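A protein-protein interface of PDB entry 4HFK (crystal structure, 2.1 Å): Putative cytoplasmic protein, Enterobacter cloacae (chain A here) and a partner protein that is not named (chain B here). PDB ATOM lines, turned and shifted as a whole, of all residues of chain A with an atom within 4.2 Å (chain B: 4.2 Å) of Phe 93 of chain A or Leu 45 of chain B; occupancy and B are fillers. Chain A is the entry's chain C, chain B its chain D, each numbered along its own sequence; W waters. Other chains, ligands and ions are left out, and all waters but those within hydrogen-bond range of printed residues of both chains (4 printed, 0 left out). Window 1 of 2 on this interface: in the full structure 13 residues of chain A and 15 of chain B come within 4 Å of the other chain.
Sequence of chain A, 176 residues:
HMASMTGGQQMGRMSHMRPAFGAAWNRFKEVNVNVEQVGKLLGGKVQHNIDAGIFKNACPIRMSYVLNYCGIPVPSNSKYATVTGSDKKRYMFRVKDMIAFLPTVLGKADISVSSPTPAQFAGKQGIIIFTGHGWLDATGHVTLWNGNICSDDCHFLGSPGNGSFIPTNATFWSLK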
ATOM      1  N   ILE A  54     -22.247  17.340  19.192  1.00  0.00           N
ATOM      2  CA  ILE A  54     -22.776  16.204  18.434  1.00  0.00           C
ATOM      3  C   ILE A  54     -22.061  14.876  18.773  1.00  0.00           C
ATOM      4  O   ILE A  54     -22.712  13.824  18.942  1.00  0.00           O
ATOM      5  CB  ILE A  54     -22.708  16.487  16.908  1.00  0.00           C
ATOM      6  CG1 ILE A  54     -23.638  17.650  16.521  1.00  0.00           C
ATOM      7  CG2 ILE A  54     -23.053  15.229  16.106  1.00  0.00           C
ATOM      8  CD1 ILE A  54     -23.386  18.190  15.094  1.00  0.00           C
ATOM      9  N   PHE A  55     -20.728  14.914  18.859  1.00  0.00           N
ATOM     10  CA  PHE A  55     -19.964  13.754  19.333  1.00  0.00           C
ATOM     11  C   PHE A  55     -19.787  13.847  20.843  1.00  0.00           C
ATOM     12  O   PHE A  55     -19.124  14.759  21.341  1.00  0.00           O
ATOM     13  CB  PHE A  55     -18.565  13.691  18.697  1.00  0.00           C
ATOM     14  CG  PHE A  55     -18.563  13.402  17.215  1.00  0.00           C
ATOM     15  CD1 PHE A  55     -19.733  13.040  16.547  1.00  0.00           C
ATOM     16  CD2 PHE A  55     -17.375  13.471  16.499  1.00  0.00           C
ATOM     17  CE1 PHE A  55     -19.715  12.768  15.181  1.00  0.00           C
ATOM     18  CE2 PHE A  55     -17.342  13.210  15.135  1.00  0.00           C
ATOM     19  CZ  PHE A  55     -18.508  12.864  14.471  1.00  0.00           C
ATOM     20  N   PRO A  60     -14.645   5.546  20.613  1.00  0.00           N
ATOM     21  CA  PRO A  60     -14.129   5.084  19.314  1.00  0.00           C
ATOM     22  C   PRO A  60     -13.117   6.054  18.723  1.00  0.00           C
ATOM     23  O   PRO A  60     -12.287   5.665  17.884  1.00  0.00           O
ATOM     24  CB  PRO A  60     -15.383   5.058  18.423  1.00  0.00           C
ATOM     25  CG  PRO A  60     -16.314   6.049  19.044  1.00  0.00           C
ATOM     26  CD  PRO A  60     -16.081   5.881  20.539  1.00  0.00           C
ATOM     27  N   ALA A  81     -18.379   4.748   9.498  1.00  0.00           N
ATOM     28  CA  ALA A  81     -18.521   6.194   9.365  1.00  0.00           C
ATOM     29  C   ALA A  81     -17.368   6.915  10.064  1.00  0.00           C
ATOM     30  O   ALA A  81     -17.062   6.637  11.230  1.00  0.00           O
ATOM     31  CB  ALA A  81     -19.861   6.654   9.927  1.00  0.00           C
ATOM     32  N   THR A  82     -16.724   7.835   9.351  1.00  0.00           N
ATOM     33  CA  THR A  82     -15.575   8.547   9.898  1.00  0.00           C
ATOM     34  C   THR A  82     -15.616  10.029   9.582  1.00  0.00           C
ATOM     35  O   THR A  82     -16.321  10.460   8.655  1.00  0.00           O
ATOM     36  CB  THR A  82     -14.234   8.002   9.336  1.00  0.00           C
ATOM     37  OG1 THR A  82     -14.159   8.255   7.927  1.00  0.00           O
ATOM     38  CG2 THR A  82     -14.081   6.515   9.587  1.00  0.00           C
ATOM     39  N   TYR A  91     -11.258   9.158  11.776  1.00  0.00           N
ATOM     40  CA  TYR A  91     -11.658   8.815  13.128  1.00  0.00           C
ATOM     41  C   TYR A  91     -13.100   8.319  13.102  1.00  0.00           C
ATOM     42  O   TYR A  91     -13.989   8.995  12.553  1.00  0.00           O
ATOM     43  CB  TYR A  91     -11.485  10.042  14.045  1.00  0.00           C
ATOM     44  CG  TYR A  91     -10.025  10.417  14.184  1.00  0.00           C
ATOM     45  CD1 TYR A  91      -9.262   9.907  15.228  1.00  0.00           C
ATOM     46  CD2 TYR A  91      -9.391  11.219  13.233  1.00  0.00           C
ATOM     47  CE1 TYR A  91      -7.919  10.207  15.349  1.00  0.00           C
ATOM     48  CE2 TYR A  91      -8.027  11.528  13.344  1.00  0.00           C
ATOM     49  CZ  TYR A  91      -7.306  11.015  14.408  1.00  0.00           C
ATOM     50  OH  TYR A  91      -5.963  11.290  14.550  1.00  0.00           O
ATOM     51  N   MET A  92     -13.322   7.127  13.657  1.00  0.00           N
ATOM     52  CA  MET A  92     -14.680   6.613  13.829  1.00  0.00           C
ATOM     53  C   MET A  92     -15.343   7.290  15.023  1.00  0.00           C
ATOM     54  O   MET A  92     -14.683   7.572  16.036  1.00  0.00           O
ATOM     55  CB  MET A  92     -14.667   5.104  14.032  1.00  0.00           C
ATOM     56  CG  MET A  92     -14.006   4.342  12.895  1.00  0.00           C
ATOM     57  SD  MET A  92     -14.268   2.578  13.108  1.00  0.00           S
ATOM     58  CE  MET A  92     -13.182   1.977  11.816  1.00  0.00           C
ATOM     59  N   PHE A  93     -16.641   7.555  14.908  1.00  0.00           N
ATOM     60  CA  PHE A  93     -17.376   8.196  15.996  1.00  0.00           C
ATOM     61  C   PHE A  93     -18.467   7.289  16.571  1.00  0.00           C
ATOM     62  O   PHE A  93     -19.159   7.665  17.523  1.00  0.00           O
ATOM     63  CB  PHE A  93     -17.953   9.552  15.563  1.00  0.00           C
ATOM     64  CG  PHE A  93     -18.912   9.467  14.402  1.00  0.00           C
ATOM     65  CD1 PHE A  93     -20.269   9.258  14.621  1.00  0.00           C
ATOM     66  CD2 PHE A  93     -18.455   9.599  13.092  1.00  0.00           C
ATOM     67  CE1 PHE A  93     -21.157   9.173  13.556  1.00  0.00           C
ATOM     68  CE2 PHE A  93     -19.345   9.521  12.010  1.00  0.00           C
ATOM     69  CZ  PHE A  93     -20.695   9.310  12.245  1.00  0.00           C
ATOM     70  N   ARG A  94     -18.607   6.092  16.005  1.00  0.00           N
ATOM     71  CA  ARG A  94     -19.574   5.119  16.519  1.00  0.00           C
ATOM     72  C   ARG A  94     -18.830   3.935  17.116  1.00  0.00           C
ATOM     73  O   ARG A  94     -17.977   3.323  16.452  1.00  0.00           O
ATOM     74  CB  ARG A  94     -20.534   4.646  15.423  1.00  0.00           C
ATOM     75  CG  ARG A  94     -21.390   5.746  14.801  1.00  0.00           C
ATOM     76  CD  ARG A  94     -22.619   5.178  14.096  1.00  0.00           C
ATOM     77  NE  ARG A  94     -23.571   6.249  13.766  1.00  0.00           N
ATOM     78  CZ  ARG A  94     -23.667   6.839  12.578  1.00  0.00           C
ATOM     79  NH1 ARG A  94     -22.896   6.445  11.567  1.00  0.00           N
ATOM     80  NH2 ARG A  94     -24.549   7.815  12.397  1.00  0.00           N
ATOM     81  N   VAL A  95     -19.126   3.610  18.369  1.00  0.00           N
ATOM     82  CA  VAL A  95     -18.381   2.533  19.016  1.00  0.00           C
ATOM     83  C   VAL A  95     -18.692   1.181  18.354  1.00  0.00           C
ATOM     84  O   VAL A  95     -17.844   0.287  18.319  1.00  0.00           O
ATOM     85  CB  VAL A  95     -18.612   2.491  20.548  1.00  0.00           C
ATOM     86  CG1 VAL A  95     -20.054   2.058  20.880  1.00  0.00           C
ATOM     87  CG2 VAL A  95     -17.604   1.547  21.202  1.00  0.00           C
ATOM     88  N   TRP B  18     -33.135  12.165  16.658  1.00  0.00           N
ATOM     89  CA  TRP B  18     -31.892  12.884  16.907  1.00  0.00           C
ATOM     90  C   TRP B  18     -32.154  14.377  16.740  1.00  0.00           C
ATOM     91  O   TRP B  18     -31.805  15.182  17.604  1.00  0.00           O
ATOM     92  CB  TRP B  18     -30.791  12.442  15.935  1.00  0.00           C
ATOM     93  CG  TRP B  18     -29.489  13.187  16.155  1.00  0.00           C
ATOM     94  CD1 TRP B  18     -28.480  12.836  17.010  1.00  0.00           C
ATOM     95  CD2 TRP B  18     -29.074  14.408  15.524  1.00  0.00           C
ATOM     96  NE1 TRP B  18     -27.466  13.761  16.950  1.00  0.00           N
ATOM     97  CE2 TRP B  18     -27.804  14.734  16.044  1.00  0.00           C
ATOM     98  CE3 TRP B  18     -29.651  15.254  14.566  1.00  0.00           C
ATOM     99  CZ2 TRP B  18     -27.098  15.869  15.631  1.00  0.00           C
ATOM    100  CZ3 TRP B  18     -28.948  16.388  14.161  1.00  0.00           C
ATOM    101  CH2 TRP B  18     -27.686  16.680  14.692  1.00  0.00           C
ATOM    102  N   ALA B  41     -29.661  12.518  22.362  1.00  0.00           N
ATOM    103  CA  ALA B  41     -29.337  12.658  20.946  1.00  0.00           C
ATOM    104  C   ALA B  41     -28.150  11.780  20.552  1.00  0.00           C
ATOM    105  O   ALA B  41     -28.193  11.096  19.520  1.00  0.00           O
ATOM    106  CB  ALA B  41     -29.053  14.121  20.606  1.00  0.00           C
ATOM    107  N   ALA B  42     -27.084  11.801  21.356  1.00  0.00           N
ATOM    108  CA  ALA B  42     -25.898  11.015  21.015  1.00  0.00           C
ATOM    109  C   ALA B  42     -26.232   9.529  20.940  1.00  0.00           C
ATOM    110  O   ALA B  42     -25.531   8.774  20.271  1.00  0.00           O
ATOM    111  CB  ALA B  42     -24.733  11.263  21.999  1.00  0.00           C
ATOM    112  N   ALA B  43     -27.290   9.103  21.629  1.00  0.00           N
ATOM    113  CA  ALA B  43     -27.701   7.709  21.535  1.00  0.00           C
ATOM    114  C   ALA B  43     -28.387   7.431  20.192  1.00  0.00           C
ATOM    115  O   ALA B  43     -28.177   6.380  19.583  1.00  0.00           O
ATOM    116  CB  ALA B  43     -28.600   7.307  22.709  1.00  0.00           C
ATOM    117  N   TRP B  44     -29.214   8.361  19.724  1.00  0.00           N
ATOM    118  CA  TRP B  44     -29.804   8.181  18.400  1.00  0.00           C
ATOM    119  C   TRP B  44     -28.701   8.232  17.341  1.00  0.00           C
ATOM    120  O   TRP B  44     -28.735   7.493  16.352  1.00  0.00           O
ATOM    121  CB  TRP B  44     -30.855   9.251  18.118  1.00  0.00           C
ATOM    122  CG  TRP B  44     -32.044   9.228  19.063  1.00  0.00           C
ATOM    123  CD1 TRP B  44     -32.375  10.180  19.993  1.00  0.00           C
ATOM    124  CD2 TRP B  44     -33.059   8.213  19.149  1.00  0.00           C
ATOM    125  NE1 TRP B  44     -33.534   9.815  20.650  1.00  0.00           N
ATOM    126  CE2 TRP B  44     -33.968   8.612  20.157  1.00  0.00           C
ATOM    127  CE3 TRP B  44     -33.290   7.008  18.472  1.00  0.00           C
ATOM    128  CZ2 TRP B  44     -35.103   7.848  20.493  1.00  0.00           C
ATOM    129  CZ3 TRP B  44     -34.411   6.242  18.818  1.00  0.00           C
ATOM    130  CH2 TRP B  44     -35.303   6.669  19.818  1.00  0.00           C
ATOM    131  N   LEU B  45     -27.727   9.115  17.550  1.00  0.00           N
ATOM    132  CA  LEU B  45     -26.600   9.238  16.623  1.00  0.00           C
ATOM    133  C   LEU B  45     -25.902   7.895  16.423  1.00  0.00           C
ATOM    134  O   LEU B  45     -25.631   7.486  15.287  1.00  0.00           O
ATOM    135  CB  LEU B  45     -25.587  10.279  17.135  1.00  0.00           C
ATOM    136  CG  LEU B  45     -24.270  10.299  16.346  1.00  0.00           C
ATOM    137  CD1 LEU B  45     -24.476  10.905  14.963  1.00  0.00           C
ATOM    138  CD2 LEU B  45     -23.183  11.069  17.105  1.00  0.00           C
ATOM    139  N   GLU B  46     -25.599   7.216  17.526  1.00  0.00           N
ATOM    140  CA  GLU B  46     -24.943   5.897  17.473  1.00  0.00           C
ATOM    141  C   GLU B  46     -25.797   4.858  16.726  1.00  0.00           C
ATOM    142  O   GLU B  46     -25.275   4.047  15.946  1.00  0.00           O
ATOM    143  CB  GLU B  46     -24.626   5.405  18.897  1.00  0.00           C
ATOM    144  CG  GLU B  46     -24.144   3.955  18.993  1.00  0.00           C
ATOM    145  CD  GLU B  46     -22.673   3.785  18.619  1.00  0.00           C
ATOM    146  OE1 GLU B  46     -21.936   4.800  18.598  1.00  0.00           O
ATOM    147  OE2 GLU B  46     -22.254   2.633  18.352  1.00  0.00           O
ATOM    148  N   ALA B  47     -27.110   4.895  16.944  1.00  0.00           N
ATOM    149  CA  ALA B  47     -27.996   3.897  16.323  1.00  0.00           C
ATOM    150  C   ALA B  47     -28.206   4.126  14.824  1.00  0.00           C
ATOM    151  O   ALA B  47     -28.483   3.185  14.074  1.00  0.00           O
ATOM    152  CB  ALA B  47     -29.332   3.847  17.035  1.00  0.00           C
ATOM    153  N   SER B  48     -28.088   5.379  14.395  1.00  0.00           N
ATOM    154  CA  SER B  48     -28.200   5.730  12.977  1.00  0.00           C
ATOM    155  C   SER B  48     -27.048   5.125  12.173  1.00  0.00           C
ATOM    156  O   SER B  48     -25.962   4.856  12.716  1.00  0.00           O
ATOM    157  CB  SER B  48     -28.179   7.257  12.820  1.00  0.00           C
ATOM    158  OG  SER B  48     -28.306   7.653  11.464  1.00  0.00           O
ATOM    159  N   ALA B  52     -21.616  11.323   9.212  1.00  0.00           N
ATOM    160  CA  ALA B  52     -21.572  12.455  10.136  1.00  0.00           C
ATOM    161  C   ALA B  52     -22.065  13.741   9.486  1.00  0.00           C
ATOM    162  O   ALA B  52     -22.716  14.573  10.129  1.00  0.00           O
ATOM    163  CB  ALA B  52     -20.162  12.648  10.645  1.00  0.00           C
ATOM    164  N   PHE B  55     -25.551  14.879   9.974  1.00  0.00           N
ATOM    165  CA  PHE B  55     -25.808  15.479  11.278  1.00  0.00           C
ATOM    166  C   PHE B  55     -25.247  16.903  11.386  1.00  0.00           C
ATOM    167  O   PHE B  55     -25.907  17.805  11.933  1.00  0.00           O
ATOM    168  CB  PHE B  55     -25.261  14.560  12.379  1.00  0.00           C
ATOM    169  CG  PHE B  55     -25.919  13.198  12.399  1.00  0.00           C
ATOM    170  CD1 PHE B  55     -27.077  12.984  13.144  1.00  0.00           C
ATOM    171  CD2 PHE B  55     -25.397  12.143  11.659  1.00  0.00           C
ATOM    172  CE1 PHE B  55     -27.698  11.735  13.161  1.00  0.00           C
ATOM    173  CE2 PHE B  55     -26.022  10.887  11.666  1.00  0.00           C
ATOM    174  CZ  PHE B  55     -27.170  10.688  12.417  1.00  0.00           C
HETATM  175  O   HOH W   1     -19.171  10.039   8.174  1.00  0.00           O
HETATM  176  O   HOH W   2     -19.729   5.786  20.080  1.00  0.00           O
HETATM  177  O   HOH W   3     -21.903   7.511  17.969  1.00  0.00           O
HETATM  178  O   HOH W   4     -25.426  13.692  18.948  1.00  0.00           O
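NE of Arg 94 of chain A is in hydrogen-bond range of O of Leu 45 of chain B (2.8 Å). O of Ser 48 of chain B is in hydrogen-bond range of NE of Arg 94 of chain A. N of Val 95 of chain A sits at hydrogen-bond distance from OE1 of Glu 46 of chain B.
Ile 54 of chain A touches Trp 18 of chain B (CG1 to CZ2, 3.99 Å). Leu 45 of chain B touches Ile 54 of chain A (CD2 to O, 3.3 Å). Leu 45 of chain B touches Phe 93 of chain A. Phe 93 of chain A touches Ala 52 of chain B. Arg 94 of chain A touches Glu 46 of chain B. Phe 55 of chain B touches Arg 94 of chain A.
Of the printed residues of chain A, Leu 45 of chain B touches Ile 54, Phe 93 and Arg 94. Of the printed residues of chain A, Phe 55 of chain B touches Arg 94 (3.5 Å). Of the printed residues of chain A, Trp 18 of chain B touches Ile 54 (3.99 Å). Of the printed residues of chain B, Ile 54 of chain A touches Trp 18 and Leu 45. Met 92 of chain A touches none of the printed residues of chain B.
Hydrophobic or aromatic side chains of chain B within 4 Å of the printed part of chain A: Trp 18, Leu 45, Ala 52 and Phe 55. Of the 10 printed residues of chain A, 4 touch a printed residue of chain B. Hydrophobic or aromatic side chains of chain A that line the printed part of chain B: Ile 54, Phe 93 and Val 95. Among the printed residues, 9 pairs touch across the chains.
Water W4 lies within hydrogen-bond range of the backbone carbonyl oxygen of Ile 54 of chain A (2.7 Å), the indole nitrogen of Trp 18 of chain B (2.9 Å) and the backbone NH of Ala 42 of chain B (3.5 Å). Water W3 lies within hydrogen-bond range of OE1 of Glu 46 of chain B (2.8 Å) and O of Phe 93 of chain A (2.8 Å). Water W2 lies within hydrogen-bond range of N of Val 95 of chain A, OE1 of Glu 46 of chain B and O of Phe 93 of chain A. Water W1 bridges the backbone carbonyl oxygen (O) of Thr 82 of chain A (2.9 Å) and the backbone NH (N) of Ala 52 of chain B (3.0 Å).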
